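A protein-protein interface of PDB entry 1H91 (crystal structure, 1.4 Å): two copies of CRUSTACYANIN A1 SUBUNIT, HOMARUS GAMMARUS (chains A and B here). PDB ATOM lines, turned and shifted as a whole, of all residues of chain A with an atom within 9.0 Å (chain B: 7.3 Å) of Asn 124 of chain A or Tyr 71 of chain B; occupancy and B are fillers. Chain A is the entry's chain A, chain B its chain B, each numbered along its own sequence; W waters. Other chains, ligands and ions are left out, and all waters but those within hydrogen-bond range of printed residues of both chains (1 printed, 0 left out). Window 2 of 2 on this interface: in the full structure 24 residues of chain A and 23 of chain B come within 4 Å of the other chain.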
ATOM      1  N   GLY A   9     -32.103  13.586   4.701  1.00  0.00           N
ATOM      2  CA  GLY A   9     -30.830  13.027   5.049  1.00  0.00           C
ATOM      3  C   GLY A   9     -30.173  12.099   4.054  1.00  0.00           C
ATOM      4  O   GLY A   9     -30.765  11.801   2.991  1.00  0.00           O
ATOM      5  N   ILE A 121     -30.794   6.070  -3.358  1.00  0.00           N
ATOM      6  CA  ILE A 121     -30.078   7.092  -4.101  1.00  0.00           C
ATOM      7  C   ILE A 121     -30.064   8.438  -3.371  1.00  0.00           C
ATOM      8  O   ILE A 121     -31.071   8.913  -2.847  1.00  0.00           O
ATOM      9  CB  ILE A 121     -30.768   7.362  -5.468  1.00  0.00           C
ATOM     10  CG1 ILE A 121     -31.147   6.104  -6.255  1.00  0.00           C
ATOM     11  CG2 ILE A 121     -29.898   8.303  -6.290  1.00  0.00           C
ATOM     12  CD1 ILE A 121     -32.446   5.475  -5.790  1.00  0.00           C
ATOM     13  N   ASP A 122     -28.912   9.099  -3.356  1.00  0.00           N
ATOM     14  CA  ASP A 122     -28.704  10.387  -2.764  1.00  0.00           C
ATOM     15  C   ASP A 122     -28.933  11.546  -3.739  1.00  0.00           C
ATOM     16  O   ASP A 122     -28.553  11.441  -4.917  1.00  0.00           O
ATOM     17  CB  ASP A 122     -27.277  10.506  -2.210  1.00  0.00           C
ATOM     18  CG  ASP A 122     -27.079   9.674  -0.962  1.00  0.00           C
ATOM     19  OD1 ASP A 122     -27.760   9.849   0.080  1.00  0.00           O
ATOM     20  OD2 ASP A 122     -26.215   8.768  -0.999  1.00  0.00           O
ATOM     21  N   TYR A 123     -29.535  12.618  -3.246  1.00  0.00           N
ATOM     22  CA  TYR A 123     -29.700  13.882  -3.965  1.00  0.00           C
ATOM     23  C   TYR A 123     -28.652  14.913  -3.510  1.00  0.00           C
ATOM     24  O   TYR A 123     -28.135  14.877  -2.389  1.00  0.00           O
ATOM     25  CB  TYR A 123     -31.106  14.455  -3.805  1.00  0.00           C
ATOM     26  CG  TYR A 123     -32.223  13.541  -4.292  1.00  0.00           C
ATOM     27  CD1 TYR A 123     -33.169  13.035  -3.418  1.00  0.00           C
ATOM     28  CD2 TYR A 123     -32.272  13.202  -5.647  1.00  0.00           C
ATOM     29  CE1 TYR A 123     -34.181  12.201  -3.897  1.00  0.00           C
ATOM     30  CE2 TYR A 123     -33.279  12.365  -6.131  1.00  0.00           C
ATOM     31  CZ  TYR A 123     -34.202  11.880  -5.238  1.00  0.00           C
ATOM     32  OH  TYR A 123     -35.222  11.046  -5.695  1.00  0.00           O
ATOM     33  N   ASN A 124     -28.367  15.893  -4.381  1.00  0.00           N
ATOM     34  CA  ASN A 124     -27.423  16.963  -4.036  1.00  0.00           C
ATOM     35  C   ASN A 124     -27.982  18.013  -3.057  1.00  0.00           C
ATOM     36  O   ASN A 124     -27.226  18.867  -2.595  1.00  0.00           O
ATOM     37  CB  ASN A 124     -26.900  17.616  -5.315  1.00  0.00           C
ATOM     38  CG  ASN A 124     -27.999  18.244  -6.147  1.00  0.00           C
ATOM     39  OD1 ASN A 124     -29.134  18.530  -5.723  1.00  0.00           O
ATOM     40  ND2 ASN A 124     -27.613  18.436  -7.415  1.00  0.00           N
ATOM     41  N   PHE A 125     -29.258  17.990  -2.720  1.00  0.00           N
ATOM     42  CA  PHE A 125     -29.868  18.875  -1.740  1.00  0.00           C
ATOM     43  C   PHE A 125     -30.031  18.237  -0.366  1.00  0.00           C
ATOM     44  O   PHE A 125     -30.662  18.801   0.534  1.00  0.00           O
ATOM     45  CB  PHE A 125     -31.190  19.452  -2.256  1.00  0.00           C
ATOM     46  CG  PHE A 125     -32.233  18.474  -2.743  1.00  0.00           C
ATOM     47  CD1 PHE A 125     -33.206  18.015  -1.850  1.00  0.00           C
ATOM     48  CD2 PHE A 125     -32.343  18.015  -4.024  1.00  0.00           C
ATOM     49  CE1 PHE A 125     -34.198  17.150  -2.274  1.00  0.00           C
ATOM     50  CE2 PHE A 125     -33.274  17.106  -4.482  1.00  0.00           C
ATOM     51  CZ  PHE A 125     -34.224  16.664  -3.563  1.00  0.00           C
ATOM     52  N   GLY A 126     -29.410  17.085  -0.110  1.00  0.00           N
ATOM     53  CA  GLY A 126     -29.295  16.519   1.221  1.00  0.00           C
ATOM     54  C   GLY A 126     -30.394  15.561   1.626  1.00  0.00           C
ATOM     55  O   GLY A 126     -30.464  15.115   2.790  1.00  0.00           O
ATOM     56  N   TYR A 127     -31.250  15.230   0.684  1.00  0.00           N
ATOM     57  CA  TYR A 127     -32.305  14.203   0.844  1.00  0.00           C
ATOM     58  C   TYR A 127     -31.856  12.924   0.131  1.00  0.00           C
ATOM     59  O   TYR A 127     -30.839  12.913  -0.579  1.00  0.00           O
ATOM     60  CB  TYR A 127     -33.629  14.713   0.325  1.00  0.00           C
ATOM     61  CG  TYR A 127     -34.468  15.638   1.199  1.00  0.00           C
ATOM     62  CD1 TYR A 127     -35.805  15.329   1.455  1.00  0.00           C
ATOM     63  CD2 TYR A 127     -33.916  16.801   1.750  1.00  0.00           C
ATOM     64  CE1 TYR A 127     -36.615  16.136   2.245  1.00  0.00           C
ATOM     65  CE2 TYR A 127     -34.707  17.642   2.546  1.00  0.00           C
ATOM     66  CZ  TYR A 127     -36.024  17.274   2.754  1.00  0.00           C
ATOM     67  OH  TYR A 127     -36.808  18.107   3.560  1.00  0.00           O
ATOM     68  N   HIS A 128     -32.596  11.849   0.264  1.00  0.00           N
ATOM     69  CA  HIS A 128     -32.421  10.616  -0.472  1.00  0.00           C
ATOM     70  C   HIS A 128     -33.801  10.088  -0.899  1.00  0.00           C
ATOM     71  O   HIS A 128     -34.842  10.550  -0.417  1.00  0.00           O
ATOM     72  CB  HIS A 128     -31.703   9.485   0.299  1.00  0.00           C
ATOM     73  CG  HIS A 128     -32.422   9.000   1.517  1.00  0.00           C
ATOM     74  ND1 HIS A 128     -33.177   7.869   1.748  1.00  0.00           N
ATOM     75  CD2 HIS A 128     -32.451   9.622   2.731  1.00  0.00           C
ATOM     76  CE1 HIS A 128     -33.630   7.818   3.010  1.00  0.00           C
ATOM     77  NE2 HIS A 128     -33.184   8.920   3.630  1.00  0.00           N
ATOM     78  N   LEU B  39     -26.234  22.995 -17.888  1.00  0.00           N
ATOM     79  CA  LEU B  39     -27.085  21.799 -17.762  1.00  0.00           C
ATOM     80  C   LEU B  39     -28.499  22.158 -17.291  1.00  0.00           C
ATOM     81  O   LEU B  39     -28.665  23.228 -16.688  1.00  0.00           O
ATOM     82  CB  LEU B  39     -26.472  20.774 -16.797  1.00  0.00           C
ATOM     83  CG  LEU B  39     -26.662  21.030 -15.307  1.00  0.00           C
ATOM     84  CD1 LEU B  39     -26.168  19.795 -14.563  1.00  0.00           C
ATOM     85  CD2 LEU B  39     -26.018  22.329 -14.819  1.00  0.00           C
ATOM     86  N   ASN B  41     -31.820  21.462 -14.757  1.00  0.00           N
ATOM     87  CA  ASN B  41     -31.923  21.139 -13.317  1.00  0.00           C
ATOM     88  C   ASN B  41     -31.735  19.651 -13.039  1.00  0.00           C
ATOM     89  O   ASN B  41     -32.466  18.809 -13.549  1.00  0.00           O
ATOM     90  CB  ASN B  41     -33.279  21.641 -12.842  1.00  0.00           C
ATOM     91  CG  ASN B  41     -33.551  21.540 -11.362  1.00  0.00           C
ATOM     92  OD1 ASN B  41     -32.646  21.361 -10.537  1.00  0.00           O
ATOM     93  ND2 ASN B  41     -34.849  21.663 -11.046  1.00  0.00           N
ATOM     94  N   ASN B  42     -30.703  19.325 -12.265  1.00  0.00           N
ATOM     95  CA  ASN B  42     -30.255  17.942 -12.031  1.00  0.00           C
ATOM     96  C   ASN B  42     -30.062  17.690 -10.549  1.00  0.00           C
ATOM     97  O   ASN B  42     -29.121  18.271  -9.988  1.00  0.00           O
ATOM     98  CB  ASN B  42     -28.948  17.698 -12.804  1.00  0.00           C
ATOM     99  CG  ASN B  42     -28.499  16.263 -12.867  1.00  0.00           C
ATOM    100  OD1 ASN B  42     -28.505  15.548 -11.849  1.00  0.00           O
ATOM    101  ND2 ASN B  42     -28.087  15.745 -14.010  1.00  0.00           N
ATOM    102  N   PRO B  43     -30.901  16.903  -9.881  1.00  0.00           N
ATOM    103  CA  PRO B  43     -30.766  16.692  -8.439  1.00  0.00           C
ATOM    104  C   PRO B  43     -29.753  15.618  -8.046  1.00  0.00           C
ATOM    105  O   PRO B  43     -29.614  15.309  -6.873  1.00  0.00           O
ATOM    106  CB  PRO B  43     -32.177  16.195  -8.071  1.00  0.00           C
ATOM    107  CG  PRO B  43     -32.571  15.385  -9.271  1.00  0.00           C
ATOM    108  CD  PRO B  43     -32.086  16.222 -10.442  1.00  0.00           C
ATOM    109  N   TYR B  44     -29.065  15.071  -9.055  1.00  0.00           N
ATOM    110  CA  TYR B  44     -28.094  14.008  -8.833  1.00  0.00           C
ATOM    111  C   TYR B  44     -26.647  14.489  -8.864  1.00  0.00           C
ATOM    112  O   TYR B  44     -25.788  13.970  -8.141  1.00  0.00           O
ATOM    113  CB  TYR B  44     -28.294  12.883  -9.867  1.00  0.00           C
ATOM    114  CG  TYR B  44     -29.724  12.376  -9.872  1.00  0.00           C
ATOM    115  CD1 TYR B  44     -30.506  12.506 -11.012  1.00  0.00           C
ATOM    116  CD2 TYR B  44     -30.284  11.758  -8.747  1.00  0.00           C
ATOM    117  CE1 TYR B  44     -31.811  12.035 -11.018  1.00  0.00           C
ATOM    118  CE2 TYR B  44     -31.600  11.284  -8.756  1.00  0.00           C
ATOM    119  CZ  TYR B  44     -32.346  11.432  -9.900  1.00  0.00           C
ATOM    120  OH  TYR B  44     -33.655  10.973  -9.904  1.00  0.00           O
ATOM    121  N   GLN B  45     -26.309  15.482  -9.699  1.00  0.00           N
ATOM    122  CA  GLN B  45     -24.935  15.957  -9.869  1.00  0.00           C
ATOM    123  C   GLN B  45     -24.413  16.564  -8.589  1.00  0.00           C
ATOM    124  O   GLN B  45     -24.989  17.549  -8.132  1.00  0.00           O
ATOM    125  CB  GLN B  45     -24.960  16.954 -11.023  1.00  0.00           C
ATOM    126  CG  GLN B  45     -23.806  17.912 -11.186  1.00  0.00           C
ATOM    127  CD  GLN B  45     -22.504  17.260 -11.573  1.00  0.00           C
ATOM    128  OE1 GLN B  45     -21.881  16.553 -10.779  1.00  0.00           O
ATOM    129  NE2 GLN B  45     -22.027  17.483 -12.792  1.00  0.00           N
ATOM    130  N   LEU B  46     -23.349  15.999  -8.011  1.00  0.00           N
ATOM    131  CA  LEU B  46     -22.773  16.461  -6.754  1.00  0.00           C
ATOM    132  C   LEU B  46     -21.734  17.563  -6.912  1.00  0.00           C
ATOM    133  O   LEU B  46     -21.366  18.202  -5.919  1.00  0.00           O
ATOM    134  CB  LEU B  46     -22.094  15.261  -6.066  1.00  0.00           C
ATOM    135  CG  LEU B  46     -23.096  14.193  -5.607  1.00  0.00           C
ATOM    136  CD1 LEU B  46     -22.387  13.047  -4.888  1.00  0.00           C
ATOM    137  CD2 LEU B  46     -24.151  14.816  -4.707  1.00  0.00           C
ATOM    138  N   ILE B  47     -21.249  17.808  -8.133  1.00  0.00           N
ATOM    139  CA  ILE B  47     -20.270  18.895  -8.311  1.00  0.00           C
ATOM    140  C   ILE B  47     -20.998  20.129  -8.857  1.00  0.00           C
ATOM    141  O   ILE B  47     -21.620  20.114  -9.950  1.00  0.00           O
ATOM    142  CB  ILE B  47     -19.174  18.381  -9.255  1.00  0.00           C
ATOM    143  CG1 ILE B  47     -18.654  16.990  -8.865  1.00  0.00           C
ATOM    144  CG2 ILE B  47     -18.077  19.453  -9.341  1.00  0.00           C
ATOM    145  CD1 ILE B  47     -17.696  16.443  -9.923  1.00  0.00           C
ATOM    146  N   GLU B  48     -20.952  21.242  -8.123  1.00  0.00           N
ATOM    147  CA  GLU B  48     -21.666  22.449  -8.492  1.00  0.00           C
ATOM    148  C   GLU B  48     -20.889  23.359  -9.432  1.00  0.00           C
ATOM    149  O   GLU B  48     -21.469  23.813 -10.438  1.00  0.00           O
ATOM    150  CB  GLU B  48     -22.033  23.244  -7.226  1.00  0.00           C
ATOM    151  CG  GLU B  48     -22.860  24.474  -7.547  1.00  0.00           C
ATOM    152  CD  GLU B  48     -23.154  25.403  -6.403  1.00  0.00           C
ATOM    153  OE1 GLU B  48     -24.025  26.309  -6.548  1.00  0.00           O
ATOM    154  OE2 GLU B  48     -22.533  25.306  -5.322  1.00  0.00           O
ATOM    155  N   LYS B  49     -19.625  23.630  -9.156  1.00  0.00           N
ATOM    156  CA  LYS B  49     -18.859  24.578  -9.970  1.00  0.00           C
ATOM    157  C   LYS B  49     -17.586  23.987 -10.572  1.00  0.00           C
ATOM    158  O   LYS B  49     -17.095  22.980 -10.041  1.00  0.00           O
ATOM    159  CB  LYS B  49     -18.464  25.779  -9.090  1.00  0.00           C
ATOM    160  CG  LYS B  49     -19.595  26.514  -8.393  1.00  0.00           C
ATOM    161  CD  LYS B  49     -19.080  27.644  -7.499  1.00  0.00           C
ATOM    162  CE  LYS B  49     -20.264  28.419  -6.925  1.00  0.00           C
ATOM    163  NZ  LYS B  49     -19.825  29.397  -5.874  1.00  0.00           N
ATOM    164  N   ILE B  69     -15.915  21.889  -7.558  1.00  0.00           N
ATOM    165  CA  ILE B  69     -16.276  22.321  -6.212  1.00  0.00           C
ATOM    166  C   ILE B  69     -17.689  21.836  -5.886  1.00  0.00           C
ATOM    167  O   ILE B  69     -18.632  22.071  -6.649  1.00  0.00           O
ATOM    168  CB  ILE B  69     -16.240  23.858  -6.059  1.00  0.00           C
ATOM    169  CG1 ILE B  69     -15.034  24.501  -6.733  1.00  0.00           C
ATOM    170  CG2 ILE B  69     -16.408  24.279  -4.595  1.00  0.00           C
ATOM    171  CD1 ILE B  69     -13.698  23.984  -6.284  1.00  0.00           C
ATOM    172  N   ALA B  70     -17.851  21.126  -4.783  1.00  0.00           N
ATOM    173  CA  ALA B  70     -19.143  20.567  -4.359  1.00  0.00           C
ATOM    174  C   ALA B  70     -20.056  21.628  -3.770  1.00  0.00           C
ATOM    175  O   ALA B  70     -19.631  22.785  -3.566  1.00  0.00           O
ATOM    176  CB  ALA B  70     -18.819  19.477  -3.341  1.00  0.00           C
ATOM    177  N   TYR B  71     -21.309  21.296  -3.455  1.00  0.00           N
ATOM    178  CA  TYR B  71     -22.297  22.284  -3.017  1.00  0.00           C
ATOM    179  C   TYR B  71     -21.902  22.849  -1.650  1.00  0.00           C
ATOM    180  O   TYR B  71     -22.371  23.923  -1.284  1.00  0.00           O
ATOM    181  CB  TYR B  71     -23.744  21.728  -2.972  1.00  0.00           C
ATOM    182  CG  TYR B  71     -24.337  21.725  -4.392  1.00  0.00           C
ATOM    183  CD1 TYR B  71     -24.136  20.629  -5.238  1.00  0.00           C
ATOM    184  CD2 TYR B  71     -25.061  22.785  -4.900  1.00  0.00           C
ATOM    185  CE1 TYR B  71     -24.668  20.645  -6.518  1.00  0.00           C
ATOM    186  CE2 TYR B  71     -25.605  22.819  -6.185  1.00  0.00           C
ATOM    187  CZ  TYR B  71     -25.393  21.702  -6.995  1.00  0.00           C
ATOM    188  OH  TYR B  71     -25.897  21.679  -8.282  1.00  0.00           O
ATOM    189  N   ASP B  72     -21.038  22.185  -0.901  1.00  0.00           N
ATOM    190  CA  ASP B  72     -20.612  22.653   0.429  1.00  0.00           C
ATOM    191  C   ASP B  72     -19.315  23.451   0.359  1.00  0.00           C
ATOM    192  O   ASP B  72     -18.720  23.833   1.365  1.00  0.00           O
ATOM    193  CB  ASP B  72     -20.440  21.481   1.396  1.00  0.00           C
ATOM    194  CG  ASP B  72     -19.319  20.530   1.053  1.00  0.00           C
ATOM    195  OD1 ASP B  72     -18.589  20.715   0.063  1.00  0.00           O
ATOM    196  OD2 ASP B  72     -19.140  19.519   1.781  1.00  0.00           O
ATOM    197  N   GLY B  73     -18.837  23.719  -0.853  1.00  0.00           N
ATOM    198  CA  GLY B  73     -17.651  24.546  -1.035  1.00  0.00           C
ATOM    199  C   GLY B  73     -16.319  23.822  -1.020  1.00  0.00           C
ATOM    200  O   GLY B  73     -15.261  24.442  -1.248  1.00  0.00           O
ATOM    201  N   ASN B  74     -16.310  22.524  -0.781  1.00  0.00           N
ATOM    202  CA  ASN B  74     -15.099  21.704  -0.835  1.00  0.00           C
ATOM    203  C   ASN B  74     -14.783  21.148  -2.212  1.00  0.00           C
ATOM    204  O   ASN B  74     -15.645  20.809  -3.016  1.00  0.00           O
ATOM    205  CB  ASN B  74     -15.266  20.504   0.126  1.00  0.00           C
ATOM    206  CG  ASN B  74     -15.309  20.995   1.568  1.00  0.00           C
ATOM    207  OD1 ASN B  74     -14.467  21.810   1.934  1.00  0.00           O
ATOM    208  ND2 ASN B  74     -16.269  20.519   2.348  1.00  0.00           N
ATOM    209  N   LEU B  76     -14.013  18.247  -4.770  1.00  0.00           N
ATOM    210  CA  LEU B  76     -14.553  16.885  -4.860  1.00  0.00           C
ATOM    211  C   LEU B  76     -14.101  16.191  -6.145  1.00  0.00           C
ATOM    212  O   LEU B  76     -14.056  16.794  -7.231  1.00  0.00           O
ATOM    213  CB  LEU B  76     -16.090  16.930  -4.790  1.00  0.00           C
ATOM    214  CG  LEU B  76     -16.897  15.637  -4.957  1.00  0.00           C
ATOM    215  CD1 LEU B  76     -16.612  14.651  -3.824  1.00  0.00           C
ATOM    216  CD2 LEU B  76     -18.402  15.913  -5.025  1.00  0.00           C
HETATM  217  O   HOH W   1     -34.354   9.211  -8.195  1.00  0.00           O
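No position is printed for both chains. Of the 8 pairs that touch across the chains among the printed residues, none has its exchanged pair printed and touching as well.
Of the printed residues of chain B, Asn 124 of chain A touches Asn 42 (3.0 Å), Pro 43 (2.8 Å), Gln 45 (2.9 Å), Leu 46 (3.97 Å) and Tyr 71 (3.8 Å). Tyr 71 of chain B touches just one residue of chain A: Asn 124 (3.8 Å). Printed residues of chain A within 4 Å of Pro 43 of chain B: Tyr 123, Asn 124 and Phe 125. Printed residues of chain B within 4 Å of Tyr 123 of chain A: Pro 43 (3.2 Å) and Tyr 44 (3.3 Å). Printed residues of chain A within 4 Å of Tyr 44 of chain B: Tyr 123 (3.3 Å). Of the printed residues of chain A, Leu 46 of chain B touches Asn 124 (3.97 Å). The nearest residue of chain A that does not touch Tyr 71 of chain B is Phe 125 of chain A (6.3 Å).
Among the printed residues, pairs that only touch across the chains: Tyr 123 of chain A with Pro 43 of chain B (3.2 Å), Tyr 123 of chain A with Tyr 44 of chain B (3.3 Å), Asn 124 of chain A with Leu 46 of chain B (3.97 Å), Asn 124 of chain A with Tyr 71 of chain B (3.8 Å) and Phe 125 of chain A with Pro 43 of chain B (3.9 Å).
ND2 of Asn 124 of chain A is in hydrogen-bond range of O of Asn 42 of chain B. O of Pro 43 of chain B sits at hydrogen-bond distance from N of Asn 124 of chain A (2.8 Å). The backbone carbonyl oxygen (O) of Gln 45 of chain B sits at hydrogen-bond distance from the side-chain amide nitrogen (ND2) of Asn 124 of chain A (2.9 Å).
Water W1 lies within hydrogen-bond range of OH of Tyr 44 of chain B (2.6 Å) and OH of Tyr 123 of chain A (3.2 Å).
Of the 17 printed residues of chain B, 6 touch a printed residue of chain A. Printed residues of chain B that touch a printed residue of chain A: Asn 42, Pro 43, Tyr 44, Gln 45, Leu 46 and Tyr 71. Of the 9 printed residues of chain A, 3 touch a printed residue of chain B. Printed residues of chain A that touch a printed residue of chain B: Tyr 123, Asn 124 and Phe 125. Among the printed residues, no Asp or Glu carboxylate lies within 4 Å of a Lys or Arg side-chain nitrogen of the other chain.
N of Tyr 44 of chain B lies within hydrogen-bond range of OD1 of Asn 42 of chain B, 2.9 Å away. The backbone NH of Ile 47 of chain B sits at hydrogen-bond distance from the side-chain amide oxygen of Gln 45 of chain B (3.0 Å). The backbone NH (N) of Gln 45 of chain B lies within hydrogen-bond range of the side-chain amide oxygen (OD1) of Asn 42 of chain B (3.1 Å).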
